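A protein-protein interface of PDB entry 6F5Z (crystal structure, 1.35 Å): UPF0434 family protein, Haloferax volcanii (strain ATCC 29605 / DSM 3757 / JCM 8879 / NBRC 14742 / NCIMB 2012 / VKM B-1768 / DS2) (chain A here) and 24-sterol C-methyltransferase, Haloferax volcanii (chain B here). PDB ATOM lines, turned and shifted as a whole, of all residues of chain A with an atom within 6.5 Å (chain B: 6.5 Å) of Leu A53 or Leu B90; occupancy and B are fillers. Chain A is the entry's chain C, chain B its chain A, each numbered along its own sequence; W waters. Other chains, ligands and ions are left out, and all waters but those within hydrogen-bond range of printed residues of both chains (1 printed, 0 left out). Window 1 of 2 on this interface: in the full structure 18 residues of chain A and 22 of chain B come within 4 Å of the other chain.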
ATOM      1  N   MET A   1      12.379  11.611 -21.333  1.00  0.00           N
ATOM      2  CA  MET A   1      13.692  11.180 -20.828  1.00  0.00           C
ATOM      3  C   MET A   1      13.884   9.717 -21.212  1.00  0.00           C
ATOM      4  O   MET A   1      12.957   8.924 -21.082  1.00  0.00           O
ATOM      5  CB  MET A   1      13.765  11.329 -19.294  1.00  0.00           C
ATOM      6  CG  MET A   1      15.069  10.786 -18.693  1.00  0.00           C
ATOM      7  SD  MET A   1      15.182  10.934 -16.885  1.00  0.00           S
ATOM      8  CE  MET A   1      15.509  12.758 -16.682  1.00  0.00           C
ATOM      9  N   LEU A   9      17.984   7.327 -11.002  1.00  0.00           N
ATOM     10  CA  LEU A   9      17.057   8.201 -10.312  1.00  0.00           C
ATOM     11  C   LEU A   9      16.499   7.522  -9.072  1.00  0.00           C
ATOM     12  O   LEU A   9      16.369   6.298  -9.041  1.00  0.00           O
ATOM     13  CB  LEU A   9      15.894   8.595 -11.230  1.00  0.00           C
ATOM     14  CG  LEU A   9      16.263   9.395 -12.493  1.00  0.00           C
ATOM     15  CD1 LEU A   9      15.002   9.683 -13.319  1.00  0.00           C
ATOM     16  CD2 LEU A   9      16.963  10.739 -12.135  1.00  0.00           C
ATOM     17  N   CYS A  10      16.157   8.317  -8.074  1.00  0.00           N
ATOM     18  CA  CYS A  10      15.552   7.799  -6.867  1.00  0.00           C
ATOM     19  C   CYS A  10      14.589   8.801  -6.309  1.00  0.00           C
ATOM     20  O   CYS A  10      14.538   9.957  -6.738  1.00  0.00           O
ATOM     21  CB  CYS A  10      16.615   7.425  -5.846  1.00  0.00           C
ATOM     22  SG  CYS A  10      17.554   8.847  -5.254  1.00  0.00           S
ATOM     23  N   ASP A  11      13.736   8.351  -5.364  1.00  0.00           N
ATOM     24  CA  ASP A  11      12.799   9.251  -4.753  1.00  0.00           C
ATOM     25  C   ASP A  11      13.570  10.351  -4.009  1.00  0.00           C
ATOM     26  O   ASP A  11      14.410  10.037  -3.196  1.00  0.00           O
ATOM     27  CB  ASP A  11      11.935   8.464  -3.759  1.00  0.00           C
ATOM     28  CG  ASP A  11      10.700   9.180  -3.271  1.00  0.00           C
ATOM     29  OD1 ASP A  11      10.762  10.422  -3.055  1.00  0.00           O
ATOM     30  OD2 ASP A  11       9.680   8.497  -3.028  1.00  0.00           O
ATOM     31  N   PRO A  12      13.353  11.633  -4.308  1.00  0.00           N
ATOM     32  CA  PRO A  12      14.119  12.685  -3.600  1.00  0.00           C
ATOM     33  C   PRO A  12      13.865  12.721  -2.110  1.00  0.00           C
ATOM     34  O   PRO A  12      14.739  13.179  -1.378  1.00  0.00           O
ATOM     35  CB  PRO A  12      13.633  13.978  -4.255  1.00  0.00           C
ATOM     36  CG  PRO A  12      12.264  13.649  -4.834  1.00  0.00           C
ATOM     37  CD  PRO A  12      12.400  12.207  -5.285  1.00  0.00           C
ATOM     38  N   LEU A  18      12.266   4.015  -7.386  1.00  0.00           N
ATOM     39  CA  LEU A  18      11.047   4.456  -8.054  1.00  0.00           C
ATOM     40  C   LEU A  18      10.600   3.358  -9.003  1.00  0.00           C
ATOM     41  O   LEU A  18      11.419   2.706  -9.664  1.00  0.00           O
ATOM     42  CB  LEU A  18      11.296   5.722  -8.906  1.00  0.00           C
ATOM     43  CG  LEU A  18      11.703   6.936  -8.077  1.00  0.00           C
ATOM     44  CD1 LEU A  18      12.461   7.954  -8.978  1.00  0.00           C
ATOM     45  CD2 LEU A  18      10.493   7.625  -7.419  1.00  0.00           C
ATOM     46  N   LEU A  35       6.857   8.223 -12.179  1.00  0.00           N
ATOM     47  CA  LEU A  35       7.804   7.517 -11.343  1.00  0.00           C
ATOM     48  C   LEU A  35       7.176   7.493  -9.957  1.00  0.00           C
ATOM     49  O   LEU A  35       6.809   8.552  -9.443  1.00  0.00           O
ATOM     50  CB  LEU A  35       9.145   8.301 -11.329  1.00  0.00           C
ATOM     51  CG  LEU A  35       9.918   8.121 -12.629  1.00  0.00           C
ATOM     52  CD1 LEU A  35      10.978   9.242 -12.811  1.00  0.00           C
ATOM     53  CD2 LEU A  35      10.615   6.756 -12.680  1.00  0.00           C
ATOM     54  N   TYR A  44       5.645  11.066  -9.109  1.00  0.00           N
ATOM     55  CA  TYR A  44       6.450  12.092  -9.795  1.00  0.00           C
ATOM     56  C   TYR A  44       6.114  11.976 -11.278  1.00  0.00           C
ATOM     57  O   TYR A  44       6.502  10.991 -11.926  1.00  0.00           O
ATOM     58  CB  TYR A  44       7.931  11.859  -9.503  1.00  0.00           C
ATOM     59  CG  TYR A  44       8.201  11.940  -8.013  1.00  0.00           C
ATOM     60  CD1 TYR A  44       8.264  13.172  -7.364  1.00  0.00           C
ATOM     61  CD2 TYR A  44       8.421  10.790  -7.255  1.00  0.00           C
ATOM     62  CE1 TYR A  44       8.503  13.258  -5.997  1.00  0.00           C
ATOM     63  CE2 TYR A  44       8.695  10.868  -5.887  1.00  0.00           C
ATOM     64  CZ  TYR A  44       8.730  12.109  -5.262  1.00  0.00           C
ATOM     65  OH  TYR A  44       8.979  12.258  -3.907  1.00  0.00           O
ATOM     66  N   PRO A  45       5.355  12.932 -11.839  1.00  0.00           N
ATOM     67  CA  PRO A  45       4.918  12.764 -13.235  1.00  0.00           C
ATOM     68  C   PRO A  45       6.016  12.999 -14.239  1.00  0.00           C
ATOM     69  O   PRO A  45       6.891  13.828 -14.007  1.00  0.00           O
ATOM     70  CB  PRO A  45       3.813  13.806 -13.381  1.00  0.00           C
ATOM     71  CG  PRO A  45       4.251  14.928 -12.446  1.00  0.00           C
ATOM     72  CD  PRO A  45       4.873  14.197 -11.254  1.00  0.00           C
ATOM     73  N   ILE A  50       9.732  15.181 -19.473  1.00  0.00           N
ATOM     74  CA  ILE A  50      10.420  15.784 -18.345  1.00  0.00           C
ATOM     75  C   ILE A  50       9.819  15.295 -17.026  1.00  0.00           C
ATOM     76  O   ILE A  50       8.667  15.644 -16.690  1.00  0.00           O
ATOM     77  CB  ILE A  50      10.364  17.335 -18.428  1.00  0.00           C
ATOM     78  CG1 ILE A  50      11.119  17.817 -19.730  1.00  0.00           C
ATOM     79  CG2 ILE A  50      10.998  17.944 -17.144  1.00  0.00           C
ATOM     80  CD1 ILE A  50      11.055  19.310 -19.967  1.00  0.00           C
ATOM     81  N   PRO A  51      10.604  14.539 -16.225  1.00  0.00           N
ATOM     82  CA  PRO A  51      10.126  14.143 -14.909  1.00  0.00           C
ATOM     83  C   PRO A  51      10.104  15.351 -13.977  1.00  0.00           C
ATOM     84  O   PRO A  51      11.069  16.149 -13.971  1.00  0.00           O
ATOM     85  CB  PRO A  51      11.167  13.135 -14.421  1.00  0.00           C
ATOM     86  CG  PRO A  51      11.952  12.770 -15.636  1.00  0.00           C
ATOM     87  CD  PRO A  51      11.930  13.964 -16.509  1.00  0.00           C
ATOM     88  N   ASN A  52       9.045  15.462 -13.164  1.00  0.00           N
ATOM     89  CA  ASN A  52       8.989  16.502 -12.155  1.00  0.00           C
ATOM     90  C   ASN A  52       9.252  15.793 -10.840  1.00  0.00           C
ATOM     91  O   ASN A  52       8.348  15.178 -10.253  1.00  0.00           O
ATOM     92  CB  ASN A  52       7.662  17.257 -12.159  1.00  0.00           C
ATOM     93  CG  ASN A  52       7.730  18.425 -11.208  1.00  0.00           C
ATOM     94  OD1 ASN A  52       8.443  18.406 -10.196  1.00  0.00           O
ATOM     95  ND2 ASN A  52       6.946  19.453 -11.480  1.00  0.00           N
ATOM     96  N   LEU A  53      10.527  15.861 -10.391  1.00  0.00           N
ATOM     97  CA  LEU A  53      11.012  15.195  -9.201  1.00  0.00           C
ATOM     98  C   LEU A  53      11.175  16.170  -8.033  1.00  0.00           C
ATOM     99  O   LEU A  53      11.991  15.915  -7.131  1.00  0.00           O
ATOM    100  CB  LEU A  53      12.287  14.380  -9.478  1.00  0.00           C
ATOM    101  CG  LEU A  53      12.016  13.105 -10.279  1.00  0.00           C
ATOM    102  CD1 LEU A  53      13.225  12.670 -11.070  1.00  0.00           C
ATOM    103  CD2 LEU A  53      11.605  11.980  -9.372  1.00  0.00           C
ATOM    104  N   LEU A  54      10.379  17.258  -8.041  1.00  0.00           N
ATOM    105  CA  LEU A  54      10.337  18.129  -6.878  1.00  0.00           C
ATOM    106  C   LEU A  54       9.644  17.352  -5.768  1.00  0.00           C
ATOM    107  O   LEU A  54       8.661  16.639  -6.031  1.00  0.00           O
ATOM    108  CB  LEU A  54       9.501  19.391  -7.130  1.00  0.00           C
ATOM    109  CG  LEU A  54      10.117  20.442  -8.005  1.00  0.00           C
ATOM    110  CD1 LEU A  54       9.087  21.462  -8.343  1.00  0.00           C
ATOM    111  CD2 LEU A  54      11.301  21.126  -7.289  1.00  0.00           C
ATOM    112  N   PRO A  55      10.018  17.618  -4.504  1.00  0.00           N
ATOM    113  CA  PRO A  55       9.271  17.034  -3.375  1.00  0.00           C
ATOM    114  C   PRO A  55       7.807  17.439  -3.466  1.00  0.00           C
ATOM    115  O   PRO A  55       7.498  18.512  -3.995  1.00  0.00           O
ATOM    116  CB  PRO A  55       9.908  17.705  -2.155  1.00  0.00           C
ATOM    117  CG  PRO A  55      11.240  18.075  -2.584  1.00  0.00           C
ATOM    118  CD  PRO A  55      11.118  18.478  -4.020  1.00  0.00           C
ATOM    119  N   ARG A  59       4.954  21.082  -5.249  1.00  0.00           N
ATOM    120  CA  ARG A  59       4.122  20.880  -6.440  1.00  0.00           C
ATOM    121  C   ARG A  59       2.658  21.124  -6.125  1.00  0.00           C
ATOM    122  O   ARG A  59       2.217  20.788  -5.031  1.00  0.00           O
ATOM    123  CB  ARG A  59       4.311  19.468  -7.005  1.00  0.00           C
ATOM    124  CG  ARG A  59       5.682  19.241  -7.628  1.00  0.00           C
ATOM    125  CD  ARG A  59       5.755  17.933  -8.385  1.00  0.00           C
ATOM    126  NE  ARG A  59       6.024  16.795  -7.506  1.00  0.00           N
ATOM    127  CZ  ARG A  59       5.154  15.819  -7.262  1.00  0.00           C
ATOM    128  NH1 ARG A  59       3.967  15.817  -7.852  1.00  0.00           N
ATOM    129  NH2 ARG A  59       5.473  14.829  -6.442  1.00  0.00           N
ATOM    130  N   VAL B  43      25.786  15.857 -13.966  1.00  0.00           N
ATOM    131  CA  VAL B  43      24.555  16.502 -13.515  1.00  0.00           C
ATOM    132  C   VAL B  43      24.873  18.006 -13.477  1.00  0.00           C
ATOM    133  O   VAL B  43      25.882  18.405 -12.909  1.00  0.00           O
ATOM    134  CB  VAL B  43      24.140  16.013 -12.123  1.00  0.00           C
ATOM    135  CG1 VAL B  43      23.040  16.899 -11.526  1.00  0.00           C
ATOM    136  CG2 VAL B  43      23.673  14.570 -12.199  1.00  0.00           C
ATOM    137  N   THR B  47      20.328  24.250 -14.247  1.00  0.00           N
ATOM    138  CA  THR B  47      20.789  24.260 -15.622  1.00  0.00           C
ATOM    139  C   THR B  47      20.426  25.506 -16.436  1.00  0.00           C
ATOM    140  O   THR B  47      21.117  25.827 -17.404  1.00  0.00           O
ATOM    141  CB  THR B  47      20.327  22.968 -16.314  1.00  0.00           C
ATOM    142  OG1 THR B  47      21.043  22.724 -17.505  1.00  0.00           O
ATOM    143  CG2 THR B  47      18.837  22.919 -16.613  1.00  0.00           C
ATOM    144  N   PHE B  66      22.242  15.224 -17.140  1.00  0.00           N
ATOM    145  CA  PHE B  66      20.969  15.529 -16.478  1.00  0.00           C
ATOM    146  C   PHE B  66      21.009  16.994 -16.127  1.00  0.00           C
ATOM    147  O   PHE B  66      21.877  17.397 -15.351  1.00  0.00           O
ATOM    148  CB  PHE B  66      20.803  14.733 -15.192  1.00  0.00           C
ATOM    149  CG  PHE B  66      20.718  13.245 -15.415  1.00  0.00           C
ATOM    150  CD1 PHE B  66      21.865  12.484 -15.547  1.00  0.00           C
ATOM    151  CD2 PHE B  66      19.483  12.601 -15.435  1.00  0.00           C
ATOM    152  CE1 PHE B  66      21.791  11.089 -15.700  1.00  0.00           C
ATOM    153  CE2 PHE B  66      19.408  11.205 -15.543  1.00  0.00           C
ATOM    154  CZ  PHE B  66      20.552  10.467 -15.735  1.00  0.00           C
ATOM    155  N   GLY B  67      20.065  17.757 -16.667  1.00  0.00           N
ATOM    156  CA  GLY B  67      19.950  19.167 -16.345  1.00  0.00           C
ATOM    157  C   GLY B  67      18.813  19.335 -15.376  1.00  0.00           C
ATOM    158  O   GLY B  67      17.658  19.103 -15.755  1.00  0.00           O
ATOM    159  N   LEU B  68      19.152  19.678 -14.109  1.00  0.00           N
ATOM    160  CA  LEU B  68      18.153  19.823 -13.067  1.00  0.00           C
ATOM    161  C   LEU B  68      17.837  21.290 -12.822  1.00  0.00           C
ATOM    162  O   LEU B  68      18.749  22.100 -12.715  1.00  0.00           O
ATOM    163  CB  LEU B  68      18.670  19.141 -11.766  1.00  0.00           C
ATOM    164  CG  LEU B  68      17.759  19.212 -10.516  1.00  0.00           C
ATOM    165  CD1 LEU B  68      18.039  18.022  -9.580  1.00  0.00           C
ATOM    166  CD2 LEU B  68      18.017  20.548  -9.717  1.00  0.00           C
ATOM    167  N   ASP B  69      16.566  21.621 -12.669  1.00  0.00           N
ATOM    168  CA  ASP B  69      16.227  23.022 -12.356  1.00  0.00           C
ATOM    169  C   ASP B  69      14.937  23.000 -11.559  1.00  0.00           C
ATOM    170  O   ASP B  69      14.097  22.128 -11.792  1.00  0.00           O
ATOM    171  CB  ASP B  69      16.063  23.854 -13.642  1.00  0.00           C
ATOM    172  CG  ASP B  69      16.295  25.315 -13.386  1.00  0.00           C
ATOM    173  OD1 ASP B  69      15.357  25.982 -12.890  1.00  0.00           O
ATOM    174  OD2 ASP B  69      17.449  25.775 -13.594  1.00  0.00           O
ATOM    175  N   GLY B  70      14.753  23.948 -10.654  1.00  0.00           N
ATOM    176  CA  GLY B  70      13.522  24.019  -9.853  1.00  0.00           C
ATOM    177  C   GLY B  70      12.369  24.660 -10.617  1.00  0.00           C
ATOM    178  O   GLY B  70      11.209  24.639 -10.135  1.00  0.00           O
ATOM    179  N   SER B  71      12.641  25.238 -11.801  1.00  0.00           N
ATOM    180  CA  SER B  71      11.630  25.905 -12.607  1.00  0.00           C
ATOM    181  C   SER B  71      11.186  25.011 -13.780  1.00  0.00           C
ATOM    182  O   SER B  71      11.977  24.804 -14.701  1.00  0.00           O
ATOM    183  CB  SER B  71      12.182  27.211 -13.162  1.00  0.00           C
ATOM    184  OG  SER B  71      11.313  27.707 -14.168  1.00  0.00           O
ATOM    185  N   VAL B  75      13.265  24.211 -17.475  1.00  0.00           N
ATOM    186  CA  VAL B  75      13.698  22.947 -18.110  1.00  0.00           C
ATOM    187  C   VAL B  75      12.944  22.670 -19.381  1.00  0.00           C
ATOM    188  O   VAL B  75      13.531  22.038 -20.262  1.00  0.00           O
ATOM    189  CB  VAL B  75      13.793  21.662 -17.255  1.00  0.00           C
ATOM    190  CG1 VAL B  75      15.044  21.666 -16.402  1.00  0.00           C
ATOM    191  CG2 VAL B  75      12.553  21.470 -16.405  1.00  0.00           C
ATOM    192  N   SER B  88      19.233  14.869 -20.801  1.00  0.00           N
ATOM    193  CA  SER B  88      17.878  14.847 -20.265  1.00  0.00           C
ATOM    194  C   SER B  88      17.718  15.986 -19.282  1.00  0.00           C
ATOM    195  O   SER B  88      18.702  16.515 -18.770  1.00  0.00           O
ATOM    196  CB  SER B  88      17.599  13.541 -19.550  1.00  0.00           C
ATOM    197  OG  SER B  88      18.365  13.464 -18.359  1.00  0.00           O
ATOM    198  N   PHE B  89      16.486  16.373 -19.036  1.00  0.00           N
ATOM    199  CA  PHE B  89      16.160  17.468 -18.150  1.00  0.00           C
ATOM    200  C   PHE B  89      15.075  17.046 -17.203  1.00  0.00           C
ATOM    201  O   PHE B  89      14.208  16.233 -17.550  1.00  0.00           O
ATOM    202  CB  PHE B  89      15.711  18.667 -18.983  1.00  0.00           C
ATOM    203  CG  PHE B  89      16.853  19.188 -19.821  1.00  0.00           C
ATOM    204  CD1 PHE B  89      17.791  20.057 -19.278  1.00  0.00           C
ATOM    205  CD2 PHE B  89      17.032  18.748 -21.125  1.00  0.00           C
ATOM    206  CE1 PHE B  89      18.892  20.492 -20.035  1.00  0.00           C
ATOM    207  CE2 PHE B  89      18.125  19.182 -21.883  1.00  0.00           C
ATOM    208  CZ  PHE B  89      19.066  20.042 -21.334  1.00  0.00           C
ATOM    209  N   LEU B  90      15.142  17.563 -15.978  1.00  0.00           N
ATOM    210  CA  LEU B  90      14.175  17.224 -14.951  1.00  0.00           C
ATOM    211  C   LEU B  90      13.970  18.399 -14.017  1.00  0.00           C
ATOM    212  O   LEU B  90      14.878  19.240 -13.822  1.00  0.00           O
ATOM    213  CB  LEU B  90      14.619  15.984 -14.157  1.00  0.00           C
ATOM    214  CG  LEU B  90      15.904  16.107 -13.316  1.00  0.00           C
ATOM    215  CD1 LEU B  90      15.919  15.056 -12.212  1.00  0.00           C
ATOM    216  CD2 LEU B  90      17.206  15.957 -14.179  1.00  0.00           C
ATOM    217  N   VAL B  91      12.766  18.448 -13.415  1.00  0.00           N
ATOM    218  CA  VAL B  91      12.474  19.437 -12.381  1.00  0.00           C
ATOM    219  C   VAL B  91      12.923  18.823 -11.067  1.00  0.00           C
ATOM    220  O   VAL B  91      12.620  17.649 -10.781  1.00  0.00           O
ATOM    221  CB  VAL B  91      10.985  19.845 -12.335  1.00  0.00           C
ATOM    222  CG1 VAL B  91      10.824  21.161 -11.560  1.00  0.00           C
ATOM    223  CG2 VAL B  91      10.374  19.980 -13.732  1.00  0.00           C
ATOM    224  N   GLY B  92      13.663  19.598 -10.263  1.00  0.00           N
ATOM    225  CA  GLY B  92      14.140  19.094  -8.995  1.00  0.00           C
ATOM    226  C   GLY B  92      14.645  20.218  -8.132  1.00  0.00           C
ATOM    227  O   GLY B  92      14.728  21.367  -8.588  1.00  0.00           O
ATOM    228  N   ASP B  93      14.908  19.898  -6.882  1.00  0.00           N
ATOM    229  CA  ASP B  93      15.313  20.898  -5.891  1.00  0.00           C
ATOM    230  C   ASP B  93      16.684  20.584  -5.279  1.00  0.00           C
ATOM    231  O   ASP B  93      17.011  19.443  -4.969  1.00  0.00           O
ATOM    232  CB  ASP B  93      14.258  20.990  -4.770  1.00  0.00           C
ATOM    233  CG  ASP B  93      14.558  22.113  -3.785  1.00  0.00           C
ATOM    234  OD1 ASP B  93      14.478  23.312  -4.190  1.00  0.00           O
ATOM    235  OD2 ASP B  93      14.900  21.801  -2.644  1.00  0.00           O
ATOM    236  N   ASP B  96      17.235  18.214  -2.081  1.00  0.00           N
ATOM    237  CA  ASP B  96      17.155  16.746  -2.092  1.00  0.00           C
ATOM    238  C   ASP B  96      17.232  16.250  -3.500  1.00  0.00           C
ATOM    239  O   ASP B  96      16.283  16.299  -4.307  1.00  0.00           O
ATOM    240  CB  ASP B  96      15.998  16.131  -1.301  1.00  0.00           C
ATOM    241  CG  ASP B  96      16.288  15.792   0.163  1.00  0.00           C
ATOM    242  OD1 ASP B  96      17.391  15.203   0.460  1.00  0.00           O
ATOM    243  OD2 ASP B  96      15.449  16.111   1.001  1.00  0.00           O
ATOM    244  N   PRO B  98      17.493  13.896  -6.615  1.00  0.00           N
ATOM    245  CA  PRO B  98      16.861  12.608  -6.925  1.00  0.00           C
ATOM    246  C   PRO B  98      17.774  11.622  -7.641  1.00  0.00           C
ATOM    247  O   PRO B  98      17.347  10.953  -8.596  1.00  0.00           O
ATOM    248  CB  PRO B  98      15.669  13.031  -7.795  1.00  0.00           C
ATOM    249  CG  PRO B  98      16.263  14.179  -8.632  1.00  0.00           C
ATOM    250  CD  PRO B  98      17.095  14.945  -7.586  1.00  0.00           C
ATOM    251  N   PHE B  99      19.034  11.516  -7.177  1.00  0.00           N
ATOM    252  CA  PHE B  99      19.996  10.565  -7.747  1.00  0.00           C
ATOM    253  C   PHE B  99      20.528   9.626  -6.679  1.00  0.00           C
ATOM    254  O   PHE B  99      20.707  10.028  -5.508  1.00  0.00           O
ATOM    255  CB  PHE B  99      21.198  11.306  -8.383  1.00  0.00           C
ATOM    256  CG  PHE B  99      20.777  12.231  -9.484  1.00  0.00           C
ATOM    257  CD1 PHE B  99      20.581  11.752 -10.775  1.00  0.00           C
ATOM    258  CD2 PHE B  99      20.572  13.574  -9.239  1.00  0.00           C
ATOM    259  CE1 PHE B  99      20.179  12.609 -11.786  1.00  0.00           C
ATOM    260  CE2 PHE B  99      20.143  14.426 -10.263  1.00  0.00           C
ATOM    261  CZ  PHE B  99      19.915  13.917 -11.512  1.00  0.00           C
HETATM  262  O   HOH W   1      14.283  17.250  -6.165  1.00  0.00           O
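The backbone carbonyl oxygen (O) of Val B91 lies within hydrogen-bond range of the backbone NH (N) of Leu A53 (2.8 Å).
O of Phe B99 is in hydrogen-bond range of SG of Cys A10 (3.4 Å).
The backbone NH of Val B91 sits at hydrogen-bond distance from the backbone carbonyl oxygen of Pro A51, at 2.9 Å.
The backbone carbonyl oxygen (O) of Pro B98 is in hydrogen-bond range of the backbone NH (N) of Cys A10.
Hydrophobic or aromatic side chains of chain A within 4 Å of the printed part of chain B: Met A1, Leu A9, Pro A12, Ile A50, Pro A51, Leu A53 and Leu A54.
Of the 18 printed residues of chain B, 10 touch a printed residue of chain A.
Hydrophobic or aromatic side chains of chain B that line the printed part of chain A: Val B75, Leu B90, Val B91, Pro B98 and Phe B99.
The backbone NH (N) of Gly B67 sits at hydrogen-bond distance from the backbone carbonyl oxygen (O) of Ser B88 (2.8 Å).
O of Gly B67 is in hydrogen-bond range of N of Leu B90.
The backbone NH of Gly B70 sits close to the backbone carbonyl oxygen of Gly B92 (3.3 Å).
The guanidinium group of Arg A59 lies within hydrogen-bond range of the backbone carbonyl oxygen of Leu A54 (3.0 Å).
N of Asp B69 is in hydrogen-bond range of O of Leu B90.
The backbone NH (N) of Gly B92 is in hydrogen-bond range of the backbone carbonyl oxygen (O) of Asp B69 (3.0 Å).
Of the printed residues of chain B, Leu A53 touches Leu B90 (3.8 Å) and Val B91 (2.8 Å).
Leu B90 touches three residues of chain A.
Of the printed residues of chain A, Phe B99 touches Leu A9 (3.7 Å) and Cys A10 (3.4 Å).
Printed residues of chain B within 4 Å of Asn A52: Val B91.
Of the printed residues of chain B, Ile A50 touches Val B75 (3.7 Å), Phe B89 (3.7 Å) and Leu B90 (3.9 Å).
The nearest printed residue of chain B that does not touch Leu A53 is Pro B98 (4.01 Å).
The nearest printed residue of chain A that does not touch Gly B92 is Leu A53 (4.3 Å).
Among the printed residues, merely in contact across the chains: Met A1 with Ser B88, Met A1 with Phe B89, Leu A9 with Pro B98, Leu A9 with Phe B99, Pro A12 with Asp B96, Ile A50 with Val B75, Ile A50 with Phe B89, Ile A50 with Leu B90, Pro A51 with Phe B89, Pro A51 with Leu B90, Asn A52 with Val B91, Leu A53 with Leu B90, Leu A54 with Val B91, Leu A54 with Gly B92 and Leu A54 with Asp B93.
Water W1 lies within hydrogen-bond range of N of Asp B93 (2.8 Å), O of Leu A53 (2.8 Å) and O of Asp B96 (2.9 Å).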
